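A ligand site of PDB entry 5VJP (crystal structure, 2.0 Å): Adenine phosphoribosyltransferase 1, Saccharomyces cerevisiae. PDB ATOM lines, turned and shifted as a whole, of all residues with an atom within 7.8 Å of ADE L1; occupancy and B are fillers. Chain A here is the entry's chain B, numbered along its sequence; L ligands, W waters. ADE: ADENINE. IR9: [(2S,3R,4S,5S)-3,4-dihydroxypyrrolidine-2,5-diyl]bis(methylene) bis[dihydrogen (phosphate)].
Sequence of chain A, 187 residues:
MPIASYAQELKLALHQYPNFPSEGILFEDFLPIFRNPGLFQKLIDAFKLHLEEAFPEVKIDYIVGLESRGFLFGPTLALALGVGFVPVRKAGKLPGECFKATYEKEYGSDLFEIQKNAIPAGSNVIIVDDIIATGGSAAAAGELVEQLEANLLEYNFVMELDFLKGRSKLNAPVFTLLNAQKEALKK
O of Leu 26 sits at hydrogen-bond distance from N6 of ADE L1, 2.7 Å away. A nitrogen (N3) of ADE L1 sits at hydrogen-bond distance from the guanidinium group (NH1) of Arg 69 (3.2 Å). A nitrogen (N1) of ADE L1 is in hydrogen-bond range of the backbone NH (N) of Glu 28 (3.2 Å). The guanidinium group (NH2) of Arg 69 is in salt-bridge range of an oxygen (O5P) of IR9 L2 (3.7 Å). An oxygen (O1P) of IR9 L2 lies within hydrogen-bond range of the backbone NH (N) of Ala 133, at 2.9 Å. An oxygen (O4) of IR9 L2 lies within hydrogen-bond range of the side-chain carboxylate (OD1) of Asp 130, 2.6 Å away. O2P of IR9 L2 sits at hydrogen-bond distance from N of Thr 134, at 3.0 Å. OG1 of Thr 134 lies within hydrogen-bond range of O2P of IR9 L2 (2.5 Å).
The guanidinium group (NH1) of Arg 69 lies within salt-bridge range of the side-chain carboxylate (OD2) of Asp 130 (2.7 Å). O of Ile 132 is in hydrogen-bond range of N of Leu 161 (3.1 Å). The backbone carbonyl oxygen (O) of Phe 27 is in hydrogen-bond range of the backbone NH (N) of Tyr 17 (3.0 Å).
CA of Phe 27 touches N1 of ADE L1, at 3.6 Å. Ile 131 touches ADE L1 (CG2 to N3, 3.6 Å). Ala 133 touches ADE L1. CD1 of Leu 161 touches N6 of ADE L1 (3.6 Å). Seven residues have an atom within 4 Å of ADE L1: Leu 26, Phe 27, Glu 28, Arg 69, Ile 131, Ala 133 and Leu 161.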
ATOM      1  N   TYR A  17     -22.337 -12.864  14.049  1.00  0.00           N
ATOM      2  CA  TYR A  17     -23.292 -11.852  14.550  1.00  0.00           C
ATOM      3  C   TYR A  17     -24.286 -11.468  13.453  1.00  0.00           C
ATOM      4  O   TYR A  17     -23.974 -10.621  12.610  1.00  0.00           O
ATOM      5  CB  TYR A  17     -22.567 -10.625  15.078  1.00  0.00           C
ATOM      6  CG  TYR A  17     -21.803 -10.885  16.357  1.00  0.00           C
ATOM      7  CD1 TYR A  17     -22.435 -10.814  17.586  1.00  0.00           C
ATOM      8  CD2 TYR A  17     -20.441 -11.215  16.326  1.00  0.00           C
ATOM      9  CE1 TYR A  17     -21.739 -11.052  18.769  1.00  0.00           C
ATOM     10  CE2 TYR A  17     -19.740 -11.455  17.496  1.00  0.00           C
ATOM     11  CZ  TYR A  17     -20.390 -11.378  18.711  1.00  0.00           C
ATOM     12  OH  TYR A  17     -19.706 -11.616  19.875  1.00  0.00           O
ATOM     13  N   PHE A  20     -25.523  -7.381  11.725  1.00  0.00           N
ATOM     14  CA  PHE A  20     -24.599  -6.311  12.112  1.00  0.00           C
ATOM     15  C   PHE A  20     -23.625  -6.090  10.942  1.00  0.00           C
ATOM     16  O   PHE A  20     -23.140  -7.075  10.381  1.00  0.00           O
ATOM     17  CB  PHE A  20     -23.845  -6.683  13.380  1.00  0.00           C
ATOM     18  CG  PHE A  20     -23.055  -5.536  13.959  1.00  0.00           C
ATOM     19  CD1 PHE A  20     -23.655  -4.615  14.792  1.00  0.00           C
ATOM     20  CD2 PHE A  20     -21.706  -5.370  13.623  1.00  0.00           C
ATOM     21  CE1 PHE A  20     -22.936  -3.543  15.304  1.00  0.00           C
ATOM     22  CE2 PHE A  20     -20.980  -4.303  14.130  1.00  0.00           C
ATOM     23  CZ  PHE A  20     -21.591  -3.387  14.975  1.00  0.00           C
ATOM     24  N   PRO A  21     -23.323  -4.850  10.566  1.00  0.00           N
ATOM     25  CA  PRO A  21     -23.840  -3.598  11.167  1.00  0.00           C
ATOM     26  C   PRO A  21     -25.305  -3.238  10.825  1.00  0.00           C
ATOM     27  O   PRO A  21     -25.895  -2.411  11.517  1.00  0.00           O
ATOM     28  CB  PRO A  21     -22.903  -2.521  10.605  1.00  0.00           C
ATOM     29  CG  PRO A  21     -22.414  -3.091   9.310  1.00  0.00           C
ATOM     30  CD  PRO A  21     -22.296  -4.578   9.536  1.00  0.00           C
ATOM     31  N   GLY A  24     -29.456  -7.964   7.200  1.00  0.00           N
ATOM     32  CA  GLY A  24     -28.983  -8.811   6.108  1.00  0.00           C
ATOM     33  C   GLY A  24     -27.513  -9.193   6.137  1.00  0.00           C
ATOM     34  O   GLY A  24     -27.148 -10.257   5.644  1.00  0.00           O
ATOM     35  N   ILE A  25     -26.676  -8.335   6.729  1.00  0.00           N
ATOM     36  CA  ILE A  25     -25.235  -8.555   6.755  1.00  0.00           C
ATOM     37  C   ILE A  25     -24.896  -9.522   7.894  1.00  0.00           C
ATOM     38  O   ILE A  25     -25.357  -9.345   9.030  1.00  0.00           O
ATOM     39  CB  ILE A  25     -24.455  -7.225   6.932  1.00  0.00           C
ATOM     40  CG1 ILE A  25     -24.796  -6.255   5.785  1.00  0.00           C
ATOM     41  CG2 ILE A  25     -22.954  -7.487   6.970  1.00  0.00           C
ATOM     42  CD1 ILE A  25     -24.352  -4.821   6.018  1.00  0.00           C
ATOM     43  N   LEU A  26     -24.109 -10.547   7.579  1.00  0.00           N
ATOM     44  CA  LEU A  26     -23.607 -11.490   8.582  1.00  0.00           C
ATOM     45  C   LEU A  26     -22.167 -11.111   8.933  1.00  0.00           C
ATOM     46  O   LEU A  26     -21.271 -11.212   8.087  1.00  0.00           O
ATOM     47  CB  LEU A  26     -23.660 -12.915   8.044  1.00  0.00           C
ATOM     48  CG  LEU A  26     -23.240 -14.022   9.013  1.00  0.00           C
ATOM     49  CD1 LEU A  26     -24.209 -14.112  10.179  1.00  0.00           C
ATOM     50  CD2 LEU A  26     -23.141 -15.365   8.288  1.00  0.00           C
ATOM     51  N   PHE A  27     -21.952 -10.665  10.173  1.00  0.00           N
ATOM     52  CA  PHE A  27     -20.631 -10.208  10.623  1.00  0.00           C
ATOM     53  C   PHE A  27     -19.825 -11.402  11.149  1.00  0.00           C
ATOM     54  O   PHE A  27     -20.265 -12.114  12.048  1.00  0.00           O
ATOM     55  CB  PHE A  27     -20.765  -9.153  11.718  1.00  0.00           C
ATOM     56  CG  PHE A  27     -19.548  -8.286  11.897  1.00  0.00           C
ATOM     57  CD1 PHE A  27     -18.507  -8.672  12.746  1.00  0.00           C
ATOM     58  CD2 PHE A  27     -19.442  -7.076  11.216  1.00  0.00           C
ATOM     59  CE1 PHE A  27     -17.389  -7.875  12.900  1.00  0.00           C
ATOM     60  CE2 PHE A  27     -18.324  -6.266  11.376  1.00  0.00           C
ATOM     61  CZ  PHE A  27     -17.296  -6.667  12.223  1.00  0.00           C
ATOM     62  N   GLU A  28     -18.653 -11.618  10.559  1.00  0.00           N
ATOM     63  CA  GLU A  28     -17.688 -12.605  11.026  1.00  0.00           C
ATOM     64  C   GLU A  28     -16.722 -11.880  11.962  1.00  0.00           C
ATOM     65  O   GLU A  28     -15.897 -11.070  11.500  1.00  0.00           O
ATOM     66  CB  GLU A  28     -16.909 -13.184   9.848  1.00  0.00           C
ATOM     67  CG  GLU A  28     -17.734 -13.969   8.826  1.00  0.00           C
ATOM     68  CD  GLU A  28     -18.246 -15.291   9.360  1.00  0.00           C
ATOM     69  OE1 GLU A  28     -17.638 -15.832  10.309  1.00  0.00           O
ATOM     70  OE2 GLU A  28     -19.254 -15.785   8.820  1.00  0.00           O
ATOM     71  N   ASP A  29     -16.828 -12.146  13.265  1.00  0.00           N
ATOM     72  CA  ASP A  29     -15.962 -11.516  14.257  1.00  0.00           C
ATOM     73  C   ASP A  29     -14.771 -12.432  14.535  1.00  0.00           C
ATOM     74  O   ASP A  29     -14.920 -13.484  15.147  1.00  0.00           O
ATOM     75  CB  ASP A  29     -16.735 -11.233  15.557  1.00  0.00           C
ATOM     76  CG  ASP A  29     -15.935 -10.396  16.563  1.00  0.00           C
ATOM     77  OD1 ASP A  29     -14.971  -9.696  16.172  1.00  0.00           O
ATOM     78  OD2 ASP A  29     -16.297 -10.428  17.765  1.00  0.00           O
ATOM     79  N   PHE A  30     -13.591 -12.023  14.066  1.00  0.00           N
ATOM     80  CA  PHE A  30     -12.327 -12.725  14.367  1.00  0.00           C
ATOM     81  C   PHE A  30     -11.634 -12.290  15.683  1.00  0.00           C
ATOM     82  O   PHE A  30     -10.604 -12.861  16.057  1.00  0.00           O
ATOM     83  CB  PHE A  30     -11.368 -12.701  13.154  1.00  0.00           C
ATOM     84  CG  PHE A  30     -10.580 -11.412  12.954  1.00  0.00           C
ATOM     85  CD1 PHE A  30     -11.020 -10.167  13.409  1.00  0.00           C
ATOM     86  CD2 PHE A  30      -9.382 -11.469  12.244  1.00  0.00           C
ATOM     87  CE1 PHE A  30     -10.276  -9.013  13.199  1.00  0.00           C
ATOM     88  CE2 PHE A  30      -8.633 -10.318  12.021  1.00  0.00           C
ATOM     89  CZ  PHE A  30      -9.079  -9.085  12.506  1.00  0.00           C
ATOM     90  N   ARG A  69      -8.533  -3.247  10.975  1.00  0.00           N
ATOM     91  CA  ARG A  69      -8.424  -4.623  11.483  1.00  0.00           C
ATOM     92  C   ARG A  69      -7.210  -5.417  10.957  1.00  0.00           C
ATOM     93  O   ARG A  69      -6.773  -6.376  11.592  1.00  0.00           O
ATOM     94  CB  ARG A  69      -9.718  -5.397  11.242  1.00  0.00           C
ATOM     95  CG  ARG A  69     -10.742  -5.210  12.348  1.00  0.00           C
ATOM     96  CD  ARG A  69     -12.039  -5.943  12.046  1.00  0.00           C
ATOM     97  NE  ARG A  69     -13.051  -5.065  11.435  1.00  0.00           N
ATOM     98  CZ  ARG A  69     -14.068  -5.489  10.671  1.00  0.00           C
ATOM     99  NH1 ARG A  69     -14.223  -6.774  10.341  1.00  0.00           N
ATOM    100  NH2 ARG A  69     -14.926  -4.597  10.202  1.00  0.00           N
ATOM    101  N   ASP A 130      -8.009  -8.261   7.440  1.00  0.00           N
ATOM    102  CA  ASP A 130      -8.859  -9.267   8.075  1.00  0.00           C
ATOM    103  C   ASP A 130      -9.726  -9.999   7.053  1.00  0.00           C
ATOM    104  O   ASP A 130      -9.715 -11.220   6.982  1.00  0.00           O
ATOM    105  CB  ASP A 130      -9.689  -8.678   9.226  1.00  0.00           C
ATOM    106  CG  ASP A 130     -10.772  -7.694   8.779  1.00  0.00           C
ATOM    107  OD1 ASP A 130     -10.490  -6.830   7.908  1.00  0.00           O
ATOM    108  OD2 ASP A 130     -11.910  -7.782   9.290  1.00  0.00           O
ATOM    109  N   ILE A 131     -10.419  -9.236   6.207  1.00  0.00           N
ATOM    110  CA  ILE A 131     -11.446  -9.793   5.323  1.00  0.00           C
ATOM    111  C   ILE A 131     -11.486  -9.050   3.988  1.00  0.00           C
ATOM    112  O   ILE A 131     -11.209  -7.854   3.936  1.00  0.00           O
ATOM    113  CB  ILE A 131     -12.824  -9.788   6.016  1.00  0.00           C
ATOM    114  CG1 ILE A 131     -13.845 -10.642   5.254  1.00  0.00           C
ATOM    115  CG2 ILE A 131     -13.340  -8.361   6.198  1.00  0.00           C
ATOM    116  CD1 ILE A 131     -15.103 -10.922   6.031  1.00  0.00           C
ATOM    117  N   ILE A 132     -11.787  -9.785   2.921  1.00  0.00           N
ATOM    118  CA  ILE A 132     -12.053  -9.183   1.613  1.00  0.00           C
ATOM    119  C   ILE A 132     -13.545  -9.377   1.329  1.00  0.00           C
ATOM    120  O   ILE A 132     -14.066 -10.482   1.420  1.00  0.00           O
ATOM    121  CB  ILE A 132     -11.151  -9.772   0.486  1.00  0.00           C
ATOM    122  CG1 ILE A 132     -11.569  -9.239  -0.887  1.00  0.00           C
ATOM    123  CG2 ILE A 132     -11.123 -11.292   0.490  1.00  0.00           C
ATOM    124  CD1 ILE A 132     -10.473  -9.312  -1.932  1.00  0.00           C
ATOM    125  N   ALA A 133     -14.227  -8.267   1.047  1.00  0.00           N
ATOM    126  CA  ALA A 133     -15.661  -8.258   0.776  1.00  0.00           C
ATOM    127  C   ALA A 133     -15.860  -7.893  -0.693  1.00  0.00           C
ATOM    128  O   ALA A 133     -15.824  -8.790  -1.551  1.00  0.00           O
ATOM    129  CB  ALA A 133     -16.381  -7.287   1.719  1.00  0.00           C
ATOM    130  N   THR A 134     -16.025  -6.606  -1.010  1.00  0.00           N
ATOM    131  CA  THR A 134     -16.137  -6.156  -2.401  1.00  0.00           C
ATOM    132  C   THR A 134     -14.790  -6.143  -3.123  1.00  0.00           C
ATOM    133  O   THR A 134     -14.750  -6.167  -4.360  1.00  0.00           O
ATOM    134  CB  THR A 134     -16.735  -4.729  -2.520  1.00  0.00           C
ATOM    135  OG1 THR A 134     -15.813  -3.776  -1.980  1.00  0.00           O
ATOM    136  CG2 THR A 134     -18.075  -4.627  -1.797  1.00  0.00           C
ATOM    137  N   MET A 159     -10.326 -13.998   6.264  1.00  0.00           N
ATOM    138  CA  MET A 159     -11.623 -14.437   5.737  1.00  0.00           C
ATOM    139  C   MET A 159     -11.861 -13.847   4.350  1.00  0.00           C
ATOM    140  O   MET A 159     -11.244 -12.851   3.976  1.00  0.00           O
ATOM    141  CB  MET A 159     -12.747 -14.012   6.690  1.00  0.00           C
ATOM    142  CG  MET A 159     -12.686 -14.671   8.064  1.00  0.00           C
ATOM    143  SD  MET A 159     -13.468 -13.718   9.374  1.00  0.00           S
ATOM    144  CE  MET A 159     -12.399 -12.309   9.548  1.00  0.00           C
ATOM    145  N   LEU A 161     -15.386 -13.262   1.643  1.00  0.00           N
ATOM    146  CA  LEU A 161     -16.793 -13.412   1.277  1.00  0.00           C
ATOM    147  C   LEU A 161     -16.868 -13.737  -0.220  1.00  0.00           C
ATOM    148  O   LEU A 161     -16.907 -12.832  -1.064  1.00  0.00           O
ATOM    149  CB  LEU A 161     -17.564 -12.135   1.634  1.00  0.00           C
ATOM    150  CG  LEU A 161     -17.442 -11.712   3.102  1.00  0.00           C
ATOM    151  CD1 LEU A 161     -18.104 -10.360   3.305  1.00  0.00           C
ATOM    152  CD2 LEU A 161     -18.055 -12.748   4.028  1.00  0.00           C
ATOM    153  N   PHE A 163     -19.075 -14.972  -2.319  1.00  0.00           N
ATOM    154  CA  PHE A 163     -20.246 -14.472  -3.064  1.00  0.00           C
ATOM    155  C   PHE A 163     -20.118 -13.048  -3.595  1.00  0.00           C
ATOM    156  O   PHE A 163     -20.692 -12.725  -4.643  1.00  0.00           O
ATOM    157  CB  PHE A 163     -21.544 -14.629  -2.235  1.00  0.00           C
ATOM    158  CG  PHE A 163     -21.540 -13.913  -0.905  1.00  0.00           C
ATOM    159  CD1 PHE A 163     -21.970 -12.588  -0.821  1.00  0.00           C
ATOM    160  CD2 PHE A 163     -21.127 -14.557   0.257  1.00  0.00           C
ATOM    161  CE1 PHE A 163     -21.976 -11.927   0.400  1.00  0.00           C
ATOM    162  CE2 PHE A 163     -21.126 -13.889   1.480  1.00  0.00           C
ATOM    163  CZ  PHE A 163     -21.538 -12.564   1.547  1.00  0.00           C
ATOM    164  N   LEU A 164     -19.355 -12.194  -2.907  1.00  0.00           N
ATOM    165  CA  LEU A 164     -19.104 -10.812  -3.367  1.00  0.00           C
ATOM    166  C   LEU A 164     -18.083 -10.704  -4.518  1.00  0.00           C
ATOM    167  O   LEU A 164     -18.024  -9.660  -5.176  1.00  0.00           O
ATOM    168  CB  LEU A 164     -18.683  -9.916  -2.199  1.00  0.00           C
ATOM    169  CG  LEU A 164     -19.814  -9.511  -1.253  1.00  0.00           C
ATOM    170  CD1 LEU A 164     -19.278  -8.976   0.069  1.00  0.00           C
ATOM    171  CD2 LEU A 164     -20.733  -8.479  -1.915  1.00  0.00           C
HETATM  172  N9  ADE L   1     -16.410  -6.280   6.191  1.00  0.00           N
HETATM  173  C8  ADE L   1     -17.243  -6.263   5.122  1.00  0.00           C
HETATM  174  N7  ADE L   1     -18.155  -7.260   5.219  1.00  0.00           N
HETATM  175  C5  ADE L   1     -17.921  -7.928   6.353  1.00  0.00           C
HETATM  176  C6  ADE L   1     -18.522  -9.102   7.061  1.00  0.00           C
HETATM  177  N6  ADE L   1     -19.589  -9.748   6.531  1.00  0.00           N
HETATM  178  N1  ADE L   1     -17.970  -9.493   8.233  1.00  0.00           N
HETATM  179  C2  ADE L   1     -16.900  -8.851   8.772  1.00  0.00           C
HETATM  180  N3  ADE L   1     -16.316  -7.790   8.188  1.00  0.00           N
HETATM  181  C4  ADE L   1     -16.761  -7.290   6.999  1.00  0.00           C
HETATM  182  O3P IR9 L   2     -13.281  -3.059   0.241  1.00  0.00           O
HETATM  183  P1  IR9 L   2     -14.044  -4.196   0.864  1.00  0.00           P
HETATM  184  O1P IR9 L   2     -13.489  -5.526   0.455  1.00  0.00           O
HETATM  185  O2P IR9 L   2     -15.497  -4.111   0.484  1.00  0.00           O
HETATM  186  O1  IR9 L   2     -13.949  -4.080   2.459  1.00  0.00           O
HETATM  187  C1  IR9 L   2     -12.749  -4.394   3.149  1.00  0.00           C
HETATM  188  C2  IR9 L   2     -13.091  -4.570   4.621  1.00  0.00           C
HETATM  189  C3  IR9 L   2     -11.903  -4.879   5.517  1.00  0.00           C
HETATM  190  O3  IR9 L   2     -10.815  -3.995   5.225  1.00  0.00           O
HETATM  191  N1  IR9 L   2     -13.679  -3.331   5.192  1.00  0.00           N
HETATM  192  C5  IR9 L   2     -13.194  -3.250   6.587  1.00  0.00           C
HETATM  193  C4  IR9 L   2     -12.506  -4.581   6.866  1.00  0.00           C
HETATM  194  O4  IR9 L   2     -11.569  -4.490   7.940  1.00  0.00           O
HETATM  195  C6  IR9 L   2     -14.324  -2.984   7.554  1.00  0.00           C
HETATM  196  O6  IR9 L   2     -15.099  -1.902   7.041  1.00  0.00           O
HETATM  197  P2  IR9 L   2     -15.434  -0.634   7.944  1.00  0.00           P
HETATM  198  O4P IR9 L   2     -14.308   0.356   7.785  1.00  0.00           O
HETATM  199  O5P IR9 L   2     -15.552  -1.063   9.396  1.00  0.00           O
HETATM  200  O6P IR9 L   2     -16.745  -0.076   7.452  1.00  0.00           O
HETATM  201  O   HOH W   1     -21.042  -8.482   4.395  1.00  0.00           O
HETATM  202  O   HOH W   2     -19.950  -6.603   3.305  1.00  0.00           O
